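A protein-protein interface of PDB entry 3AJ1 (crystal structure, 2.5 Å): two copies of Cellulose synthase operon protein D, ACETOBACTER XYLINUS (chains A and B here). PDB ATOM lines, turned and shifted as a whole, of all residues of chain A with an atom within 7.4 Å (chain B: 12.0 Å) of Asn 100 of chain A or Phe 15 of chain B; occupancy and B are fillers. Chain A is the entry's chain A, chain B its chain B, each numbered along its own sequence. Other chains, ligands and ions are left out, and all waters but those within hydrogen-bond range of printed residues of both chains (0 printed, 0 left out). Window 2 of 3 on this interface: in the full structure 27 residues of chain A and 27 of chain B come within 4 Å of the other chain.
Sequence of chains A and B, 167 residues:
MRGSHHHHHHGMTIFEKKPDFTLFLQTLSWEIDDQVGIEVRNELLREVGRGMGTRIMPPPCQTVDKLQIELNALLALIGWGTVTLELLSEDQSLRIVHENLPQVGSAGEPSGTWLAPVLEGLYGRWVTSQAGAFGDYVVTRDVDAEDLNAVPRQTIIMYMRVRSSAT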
ATOM      1  N   GLY A  79       7.506  -0.976 -17.829  1.00  0.00           N
ATOM      2  CA  GLY A  79       7.584  -1.121 -16.383  1.00  0.00           C
ATOM      3  C   GLY A  79       6.542  -0.324 -15.616  1.00  0.00           C
ATOM      4  O   GLY A  79       6.839   0.216 -14.554  1.00  0.00           O
ATOM      5  N   TRP A  80       5.308  -0.271 -16.116  1.00  0.00           N
ATOM      6  CA  TRP A  80       4.275   0.528 -15.441  1.00  0.00           C
ATOM      7  C   TRP A  80       3.299  -0.266 -14.587  1.00  0.00           C
ATOM      8  O   TRP A  80       2.284   0.273 -14.143  1.00  0.00           O
ATOM      9  CB  TRP A  80       3.529   1.442 -16.417  1.00  0.00           C
ATOM     10  CG  TRP A  80       4.240   2.763 -16.671  1.00  0.00           C
ATOM     11  CD1 TRP A  80       5.562   2.943 -16.968  1.00  0.00           C
ATOM     12  CD2 TRP A  80       3.651   4.068 -16.669  1.00  0.00           C
ATOM     13  NE1 TRP A  80       5.833   4.272 -17.130  1.00  0.00           N
ATOM     14  CE2 TRP A  80       4.681   4.989 -16.956  1.00  0.00           C
ATOM     15  CE3 TRP A  80       2.349   4.549 -16.455  1.00  0.00           C
ATOM     16  CZ2 TRP A  80       4.455   6.368 -17.038  1.00  0.00           C
ATOM     17  CZ3 TRP A  80       2.125   5.922 -16.524  1.00  0.00           C
ATOM     18  CH2 TRP A  80       3.172   6.815 -16.820  1.00  0.00           C
ATOM     19  N   GLY A  81       3.614  -1.528 -14.335  1.00  0.00           N
ATOM     20  CA  GLY A  81       2.767  -2.360 -13.502  1.00  0.00           C
ATOM     21  C   GLY A  81       1.971  -3.390 -14.272  1.00  0.00           C
ATOM     22  O   GLY A  81       2.336  -3.787 -15.378  1.00  0.00           O
ATOM     23  N   THR A  82       0.879  -3.837 -13.661  1.00  0.00           N
ATOM     24  CA  THR A  82       0.047  -4.894 -14.223  1.00  0.00           C
ATOM     25  C   THR A  82      -1.388  -4.444 -14.095  1.00  0.00           C
ATOM     26  O   THR A  82      -1.692  -3.585 -13.277  1.00  0.00           O
ATOM     27  CB  THR A  82       0.235  -6.265 -13.488  1.00  0.00           C
ATOM     28  OG1 THR A  82       0.024  -6.095 -12.084  1.00  0.00           O
ATOM     29  CG2 THR A  82       1.632  -6.824 -13.700  1.00  0.00           C
ATOM     30  N   HIS A  98      -5.400  -1.474 -11.747  1.00  0.00           N
ATOM     31  CA  HIS A  98      -4.017  -1.341 -12.169  1.00  0.00           C
ATOM     32  C   HIS A  98      -3.111  -1.355 -10.951  1.00  0.00           C
ATOM     33  O   HIS A  98      -3.233  -0.509 -10.057  1.00  0.00           O
ATOM     34  CB  HIS A  98      -3.834  -0.025 -12.893  1.00  0.00           C
ATOM     35  CG  HIS A  98      -2.438   0.205 -13.347  1.00  0.00           C
ATOM     36  ND1 HIS A  98      -2.028  -0.046 -14.639  1.00  0.00           N
ATOM     37  CD2 HIS A  98      -1.345   0.647 -12.677  1.00  0.00           C
ATOM     38  CE1 HIS A  98      -0.743   0.239 -14.750  1.00  0.00           C
ATOM     39  NE2 HIS A  98      -0.305   0.668 -13.575  1.00  0.00           N
ATOM     40  N   GLU A  99      -2.186  -2.295 -10.932  1.00  0.00           N
ATOM     41  CA  GLU A  99      -1.283  -2.413  -9.806  1.00  0.00           C
ATOM     42  C   GLU A  99       0.096  -1.840 -10.081  1.00  0.00           C
ATOM     43  O   GLU A  99       0.624  -1.940 -11.189  1.00  0.00           O
ATOM     44  CB  GLU A  99      -1.212  -3.871  -9.344  1.00  0.00           C
ATOM     45  CG  GLU A  99      -2.334  -4.206  -8.389  1.00  0.00           C
ATOM     46  CD  GLU A  99      -2.812  -5.637  -8.498  1.00  0.00           C
ATOM     47  OE1 GLU A  99      -2.008  -6.533  -8.863  1.00  0.00           O
ATOM     48  OE2 GLU A  99      -4.013  -5.864  -8.214  1.00  0.00           O
ATOM     49  N   ASN A 100       0.664  -1.218  -9.054  1.00  0.00           N
ATOM     50  CA  ASN A 100       2.017  -0.688  -9.126  1.00  0.00           C
ATOM     51  C   ASN A 100       2.167   0.422 -10.128  1.00  0.00           C
ATOM     52  O   ASN A 100       3.052   0.361 -10.970  1.00  0.00           O
ATOM     53  CB  ASN A 100       3.031  -1.784  -9.476  1.00  0.00           C
ATOM     54  CG  ASN A 100       3.113  -2.854  -8.429  1.00  0.00           C
ATOM     55  OD1 ASN A 100       3.341  -2.571  -7.253  1.00  0.00           O
ATOM     56  ND2 ASN A 100       2.938  -4.095  -8.846  1.00  0.00           N
ATOM     57  N   LEU A 101       1.295   1.424 -10.049  1.00  0.00           N
ATOM     58  CA  LEU A 101       1.502   2.678 -10.741  1.00  0.00           C
ATOM     59  C   LEU A 101       2.849   3.255 -10.269  1.00  0.00           C
ATOM     60  O   LEU A 101       3.094   3.312  -9.063  1.00  0.00           O
ATOM     61  CB  LEU A 101       0.370   3.642 -10.375  1.00  0.00           C
ATOM     62  CG  LEU A 101       0.403   5.046 -10.993  1.00  0.00           C
ATOM     63  CD1 LEU A 101      -0.110   5.039 -12.415  1.00  0.00           C
ATOM     64  CD2 LEU A 101      -0.363   6.012 -10.108  1.00  0.00           C
ATOM     65  N   PRO A 102       3.730   3.665 -11.204  1.00  0.00           N
ATOM     66  CA  PRO A 102       5.009   4.291 -10.795  1.00  0.00           C
ATOM     67  C   PRO A 102       4.796   5.510  -9.888  1.00  0.00           C
ATOM     68  O   PRO A 102       3.932   6.348 -10.170  1.00  0.00           O
ATOM     69  CB  PRO A 102       5.636   4.719 -12.125  1.00  0.00           C
ATOM     70  CG  PRO A 102       5.024   3.771 -13.157  1.00  0.00           C
ATOM     71  CD  PRO A 102       3.615   3.542 -12.670  1.00  0.00           C
ATOM     72  N   GLN A 103       5.545   5.582  -8.790  1.00  0.00           N
ATOM     73  CA  GLN A 103       5.411   6.662  -7.823  1.00  0.00           C
ATOM     74  C   GLN A 103       6.378   7.782  -8.150  1.00  0.00           C
ATOM     75  O   GLN A 103       7.522   7.532  -8.540  1.00  0.00           O
ATOM     76  CB  GLN A 103       5.637   6.148  -6.412  1.00  0.00           C
ATOM     77  CG  GLN A 103       5.120   7.084  -5.335  1.00  0.00           C
ATOM     78  CD  GLN A 103       5.321   6.536  -3.934  1.00  0.00           C
ATOM     79  OE1 GLN A 103       6.305   6.863  -3.282  1.00  0.00           O
ATOM     80  NE2 GLN A 103       4.395   5.698  -3.468  1.00  0.00           N
ATOM     81  N   LEU A 119      -3.029   7.080 -16.889  1.00  0.00           N
ATOM     82  CA  LEU A 119      -3.710   5.814 -17.013  1.00  0.00           C
ATOM     83  C   LEU A 119      -5.149   5.933 -17.557  1.00  0.00           C
ATOM     84  O   LEU A 119      -5.558   5.140 -18.411  1.00  0.00           O
ATOM     85  CB  LEU A 119      -3.706   5.129 -15.647  1.00  0.00           C
ATOM     86  CG  LEU A 119      -2.688   3.988 -15.480  1.00  0.00           C
ATOM     87  CD1 LEU A 119      -1.314   4.283 -16.037  1.00  0.00           C
ATOM     88  CD2 LEU A 119      -2.616   3.575 -14.016  1.00  0.00           C
ATOM     89  N   PRO A 152      -3.943  -0.761  -1.750  1.00  0.00           N
ATOM     90  CA  PRO A 152      -2.601  -0.171  -1.623  1.00  0.00           C
ATOM     91  C   PRO A 152      -2.503   1.157  -2.369  1.00  0.00           C
ATOM     92  O   PRO A 152      -3.286   1.419  -3.281  1.00  0.00           O
ATOM     93  CB  PRO A 152      -1.684  -1.214  -2.273  1.00  0.00           C
ATOM     94  CG  PRO A 152      -2.438  -2.495  -2.200  1.00  0.00           C
ATOM     95  CD  PRO A 152      -3.899  -2.144  -2.268  1.00  0.00           C
ATOM     96  N   ARG A 153      -1.535   1.973  -1.978  1.00  0.00           N
ATOM     97  CA  ARG A 153      -1.360   3.330  -2.485  1.00  0.00           C
ATOM     98  C   ARG A 153      -1.240   3.441  -4.013  1.00  0.00           C
ATOM     99  O   ARG A 153      -1.744   4.400  -4.596  1.00  0.00           O
ATOM    100  CB  ARG A 153      -0.147   3.973  -1.804  1.00  0.00           C
ATOM    101  CG  ARG A 153       0.105   5.437  -2.158  1.00  0.00           C
ATOM    102  CD  ARG A 153      -1.136   6.300  -1.953  1.00  0.00           C
ATOM    103  NE  ARG A 153      -1.733   6.135  -0.627  1.00  0.00           N
ATOM    104  CZ  ARG A 153      -1.379   6.826   0.454  1.00  0.00           C
ATOM    105  NH1 ARG A 153      -0.412   7.741   0.396  1.00  0.00           N
ATOM    106  NH2 ARG A 153      -2.002   6.599   1.600  1.00  0.00           N
ATOM    107  N   GLN A 154      -0.572   2.471  -4.638  1.00  0.00           N
ATOM    108  CA  GLN A 154      -0.300   2.506  -6.064  1.00  0.00           C
ATOM    109  C   GLN A 154      -1.233   1.619  -6.904  1.00  0.00           C
ATOM    110  O   GLN A 154      -0.996   1.433  -8.103  1.00  0.00           O
ATOM    111  CB  GLN A 154       1.169   2.133  -6.351  1.00  0.00           C
ATOM    112  CG  GLN A 154       2.233   2.953  -5.600  1.00  0.00           C
ATOM    113  CD  GLN A 154       2.075   4.448  -5.742  1.00  0.00           C
ATOM    114  OE1 GLN A 154       1.995   5.153  -4.746  1.00  0.00           O
ATOM    115  NE2 GLN A 154       2.029   4.945  -6.977  1.00  0.00           N
ATOM    116  N   THR A 155      -2.265   1.053  -6.285  1.00  0.00           N
ATOM    117  CA  THR A 155      -3.304   0.394  -7.046  1.00  0.00           C
ATOM    118  C   THR A 155      -4.343   1.447  -7.434  1.00  0.00           C
ATOM    119  O   THR A 155      -4.881   2.135  -6.578  1.00  0.00           O
ATOM    120  CB  THR A 155      -3.959  -0.772  -6.284  1.00  0.00           C
ATOM    121  OG1 THR A 155      -2.976  -1.778  -6.024  1.00  0.00           O
ATOM    122  CG2 THR A 155      -5.097  -1.398  -7.110  1.00  0.00           C
ATOM    123  N   ILE A 156      -4.582   1.577  -8.739  1.00  0.00           N
ATOM    124  CA  ILE A 156      -5.538   2.532  -9.287  1.00  0.00           C
ATOM    125  C   ILE A 156      -6.733   1.767  -9.858  1.00  0.00           C
ATOM    126  O   ILE A 156      -6.570   0.920 -10.747  1.00  0.00           O
ATOM    127  CB  ILE A 156      -4.885   3.410 -10.390  1.00  0.00           C
ATOM    128  CG1 ILE A 156      -3.601   4.094  -9.865  1.00  0.00           C
ATOM    129  CG2 ILE A 156      -5.886   4.433 -10.954  1.00  0.00           C
ATOM    130  CD1 ILE A 156      -3.822   5.022  -8.684  1.00  0.00           C
ATOM    131  N   MET B  12      10.443 -17.025 -12.424  1.00  0.00           N
ATOM    132  CA  MET B  12      10.530 -16.002 -11.339  1.00  0.00           C
ATOM    133  C   MET B  12      10.845 -14.600 -11.877  1.00  0.00           C
ATOM    134  O   MET B  12      11.947 -14.343 -12.382  1.00  0.00           O
ATOM    135  CB  MET B  12      11.548 -16.419 -10.271  1.00  0.00           C
ATOM    136  CG  MET B  12      11.464 -15.572  -9.014  1.00  0.00           C
ATOM    137  SD  MET B  12       9.590 -15.022  -8.722  1.00  0.00           S
ATOM    138  CE  MET B  12       9.799 -14.058  -7.017  1.00  0.00           C
ATOM    139  N   THR B  13       9.880 -13.694 -11.718  1.00  0.00           N
ATOM    140  CA  THR B  13       9.857 -12.431 -12.455  1.00  0.00           C
ATOM    141  C   THR B  13      10.376 -11.211 -11.676  1.00  0.00           C
ATOM    142  O   THR B  13       9.993 -10.989 -10.518  1.00  0.00           O
ATOM    143  CB  THR B  13       8.419 -12.128 -12.964  1.00  0.00           C
ATOM    144  OG1 THR B  13       7.851 -13.307 -13.554  1.00  0.00           O
ATOM    145  CG2 THR B  13       8.417 -10.991 -13.989  1.00  0.00           C
ATOM    146  N   ILE B  14      11.255 -10.439 -12.325  1.00  0.00           N
ATOM    147  CA  ILE B  14      11.528  -9.064 -11.911  1.00  0.00           C
ATOM    148  C   ILE B  14      10.271  -8.269 -12.258  1.00  0.00           C
ATOM    149  O   ILE B  14       9.976  -8.050 -13.442  1.00  0.00           O
ATOM    150  CB  ILE B  14      12.719  -8.409 -12.686  1.00  0.00           C
ATOM    151  CG1 ILE B  14      14.004  -9.258 -12.628  1.00  0.00           C
ATOM    152  CG2 ILE B  14      12.964  -6.968 -12.190  1.00  0.00           C
ATOM    153  CD1 ILE B  14      15.092  -8.725 -11.683  1.00  0.00           C
ATOM    154  N   PHE B  15       9.517  -7.855 -11.241  1.00  0.00           N
ATOM    155  CA  PHE B  15       8.416  -6.922 -11.475  1.00  0.00           C
ATOM    156  C   PHE B  15       9.088  -5.576 -11.774  1.00  0.00           C
ATOM    157  O   PHE B  15       9.458  -4.828 -10.864  1.00  0.00           O
ATOM    158  CB  PHE B  15       7.392  -6.923 -10.313  1.00  0.00           C
ATOM    159  CG  PHE B  15       7.523  -5.770  -9.350  1.00  0.00           C
ATOM    160  CD1 PHE B  15       6.709  -4.645  -9.482  1.00  0.00           C
ATOM    161  CD2 PHE B  15       8.440  -5.817  -8.297  1.00  0.00           C
ATOM    162  CE1 PHE B  15       6.820  -3.570  -8.598  1.00  0.00           C
ATOM    163  CE2 PHE B  15       8.559  -4.746  -7.404  1.00  0.00           C
ATOM    164  CZ  PHE B  15       7.746  -3.619  -7.556  1.00  0.00           C
ATOM    165  N   GLU B  16       9.284  -5.319 -13.071  1.00  0.00           N
ATOM    166  CA  GLU B  16      10.238  -4.308 -13.560  1.00  0.00           C
ATOM    167  C   GLU B  16      10.225  -3.010 -12.748  1.00  0.00           C
ATOM    168  O   GLU B  16       9.440  -2.092 -13.009  1.00  0.00           O
ATOM    169  CB  GLU B  16      10.067  -4.047 -15.071  1.00  0.00           C
ATOM    170  CG  GLU B  16      11.268  -3.340 -15.737  1.00  0.00           C
ATOM    171  CD  GLU B  16      11.216  -3.344 -17.275  1.00  0.00           C
ATOM    172  OE1 GLU B  16      11.110  -4.431 -17.887  1.00  0.00           O
ATOM    173  OE2 GLU B  16      11.302  -2.253 -17.875  1.00  0.00           O
ATOM    174  N   LYS B  17      11.089  -2.980 -11.729  1.00  0.00           N
ATOM    175  CA  LYS B  17      11.377  -1.762 -10.982  1.00  0.00           C
ATOM    176  C   LYS B  17      12.404  -0.956 -11.784  1.00  0.00           C
ATOM    177  O   LYS B  17      13.274  -0.264 -11.242  1.00  0.00           O
ATOM    178  CB  LYS B  17      11.850  -2.060  -9.549  1.00  0.00           C
ATOM    179  CG  LYS B  17      12.199  -0.806  -8.718  1.00  0.00           C
ATOM    180  CD  LYS B  17      10.958  -0.054  -8.216  1.00  0.00           C
ATOM    181  CE  LYS B  17      10.902   1.400  -8.718  1.00  0.00           C
ATOM    182  NZ  LYS B  17      12.238   2.011  -9.054  1.00  0.00           N
ATOM    183  N   LYS B  18      12.311  -1.098 -13.098  1.00  0.00           N
ATOM    184  CA  LYS B  18      12.755  -0.055 -13.985  1.00  0.00           C
ATOM    185  C   LYS B  18      11.489   0.404 -14.694  1.00  0.00           C
ATOM    186  O   LYS B  18      11.196  -0.067 -15.797  1.00  0.00           O
ATOM    187  CB  LYS B  18      13.827  -0.544 -14.980  1.00  0.00           C
ATOM    188  CG  LYS B  18      15.263  -0.558 -14.418  1.00  0.00           C
ATOM    189  CD  LYS B  18      16.310  -0.579 -15.537  1.00  0.00           C
ATOM    190  CE  LYS B  18      17.738  -0.440 -14.979  1.00  0.00           C
ATOM    191  NZ  LYS B  18      18.787  -0.259 -16.044  1.00  0.00           N
ATOM    192  N   PRO B  19      10.696   1.273 -14.033  1.00  0.00           N
ATOM    193  CA  PRO B  19       9.719   2.014 -14.813  1.00  0.00           C
ATOM    194  C   PRO B  19      10.482   2.911 -15.773  1.00  0.00           C
ATOM    195  O   PRO B  19      11.388   3.629 -15.370  1.00  0.00           O
ATOM    196  CB  PRO B  19       8.977   2.862 -13.767  1.00  0.00           C
ATOM    197  CG  PRO B  19       9.259   2.228 -12.467  1.00  0.00           C
ATOM    198  CD  PRO B  19      10.602   1.589 -12.597  1.00  0.00           C
ATOM    199  N   ASP B  20      10.131   2.814 -17.042  1.00  0.00           N
ATOM    200  CA  ASP B  20      10.685   3.652 -18.075  1.00  0.00           C
ATOM    201  C   ASP B  20       9.779   4.870 -18.246  1.00  0.00           C
ATOM    202  O   ASP B  20       8.574   4.722 -18.443  1.00  0.00           O
ATOM    203  CB  ASP B  20      10.757   2.838 -19.359  1.00  0.00           C
ATOM    204  CG  ASP B  20      11.306   3.624 -20.522  1.00  0.00           C
ATOM    205  OD1 ASP B  20      12.421   4.181 -20.366  1.00  0.00           O
ATOM    206  OD2 ASP B  20      10.624   3.673 -21.594  1.00  0.00           O
ATOM    207  N   PHE B  21      10.347   6.068 -18.141  1.00  0.00           N
ATOM    208  CA  PHE B  21       9.601   7.309 -18.348  1.00  0.00           C
ATOM    209  C   PHE B  21       9.905   7.974 -19.677  1.00  0.00           C
ATOM    210  O   PHE B  21       9.362   9.036 -19.975  1.00  0.00           O
ATOM    211  CB  PHE B  21       9.860   8.308 -17.230  1.00  0.00           C
ATOM    212  CG  PHE B  21       9.408   7.841 -15.886  1.00  0.00           C
ATOM    213  CD1 PHE B  21       8.056   7.648 -15.624  1.00  0.00           C
ATOM    214  CD2 PHE B  21      10.331   7.633 -14.860  1.00  0.00           C
ATOM    215  CE1 PHE B  21       7.626   7.222 -14.377  1.00  0.00           C
ATOM    216  CE2 PHE B  21       9.908   7.211 -13.598  1.00  0.00           C
ATOM    217  CZ  PHE B  21       8.553   7.004 -13.358  1.00  0.00           C
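No position is printed for both chains. Of the 6 pairs that touch across the chains among the printed residues, none has its exchanged pair printed and touching as well.
Of chain B, only Phe 15 (3.8 Å) comes within 4 Å of Asn 100 of chain A. Of chain A, only Asn 100 (3.8 Å) comes within 4 Å of Phe 15 of chain B. Gly 79 of chain A touches just these residues of chain B: Glu 16 (3.8 Å), Lys 18 (3.8 Å) and Pro 19 (3.4 Å). No residue of chain B comes within 4 Å of Gly 81 of chain A. No residue of chain B comes within 4 Å of His 98 of chain A. No residue of chain B comes within 4 Å of Glu 99 of chain A. Leu 101 of chain A touches none of the printed residues of chain B. Pro 102 of chain A touches just one residue of chain B: Phe 21. No residue of chain B comes within 4 Å of Gln 154 of chain A. No residue of chain B comes within 4 Å of Thr 155 of chain A. Printed residues of chain A within 4 Å of Asp 20 of chain B: Trp 80 (3.1 Å). Printed residues of chain A within 4 Å of Glu 16 of chain B: Gly 79 (3.8 Å). Printed residues of chain A within 4 Å of Pro 19 of chain B: Gly 79 (3.4 Å). The nearest residue of chain A that does not touch Phe 15 of chain B is Gly 81 of chain A (6.1 Å).
NE2 of His 98 of chain A sits at hydrogen-bond distance from O of Trp 80 of chain A (2.7 Å). The backbone carbonyl oxygen of Gln 154 of chain A is in hydrogen-bond range of the backbone NH of Asn 100 of chain A, at 3.3 Å.
Glu 16 of chain B touches Gly 79 of chain A (O to O, 3.8 Å). Gly 79 of chain A touches Lys 18 of chain B. Pro 19 of chain B touches Gly 79 of chain A (CA to O, 3.4 Å). Phe 15 of chain B touches Asn 100 of chain A (CE1 to CG, 3.8 Å). Pro 102 of chain A touches Phe 21 of chain B (CB to CZ, 3.9 Å).
O of Asp 20 of chain B lies within hydrogen-bond range of NE1 of Trp 80 of chain A, 3.1 Å away.
Hydrophobic or aromatic side chains of chain B that line the printed part of chain A: Phe 15, Pro 19 and Phe 21. Hydrophobic or aromatic side chains of chain A that line the printed part of chain B: Trp 80 and Pro 102. Among the printed residues, no Asp or Glu carboxylate lies within 4 Å of a Lys or Arg side-chain nitrogen of the other chain.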
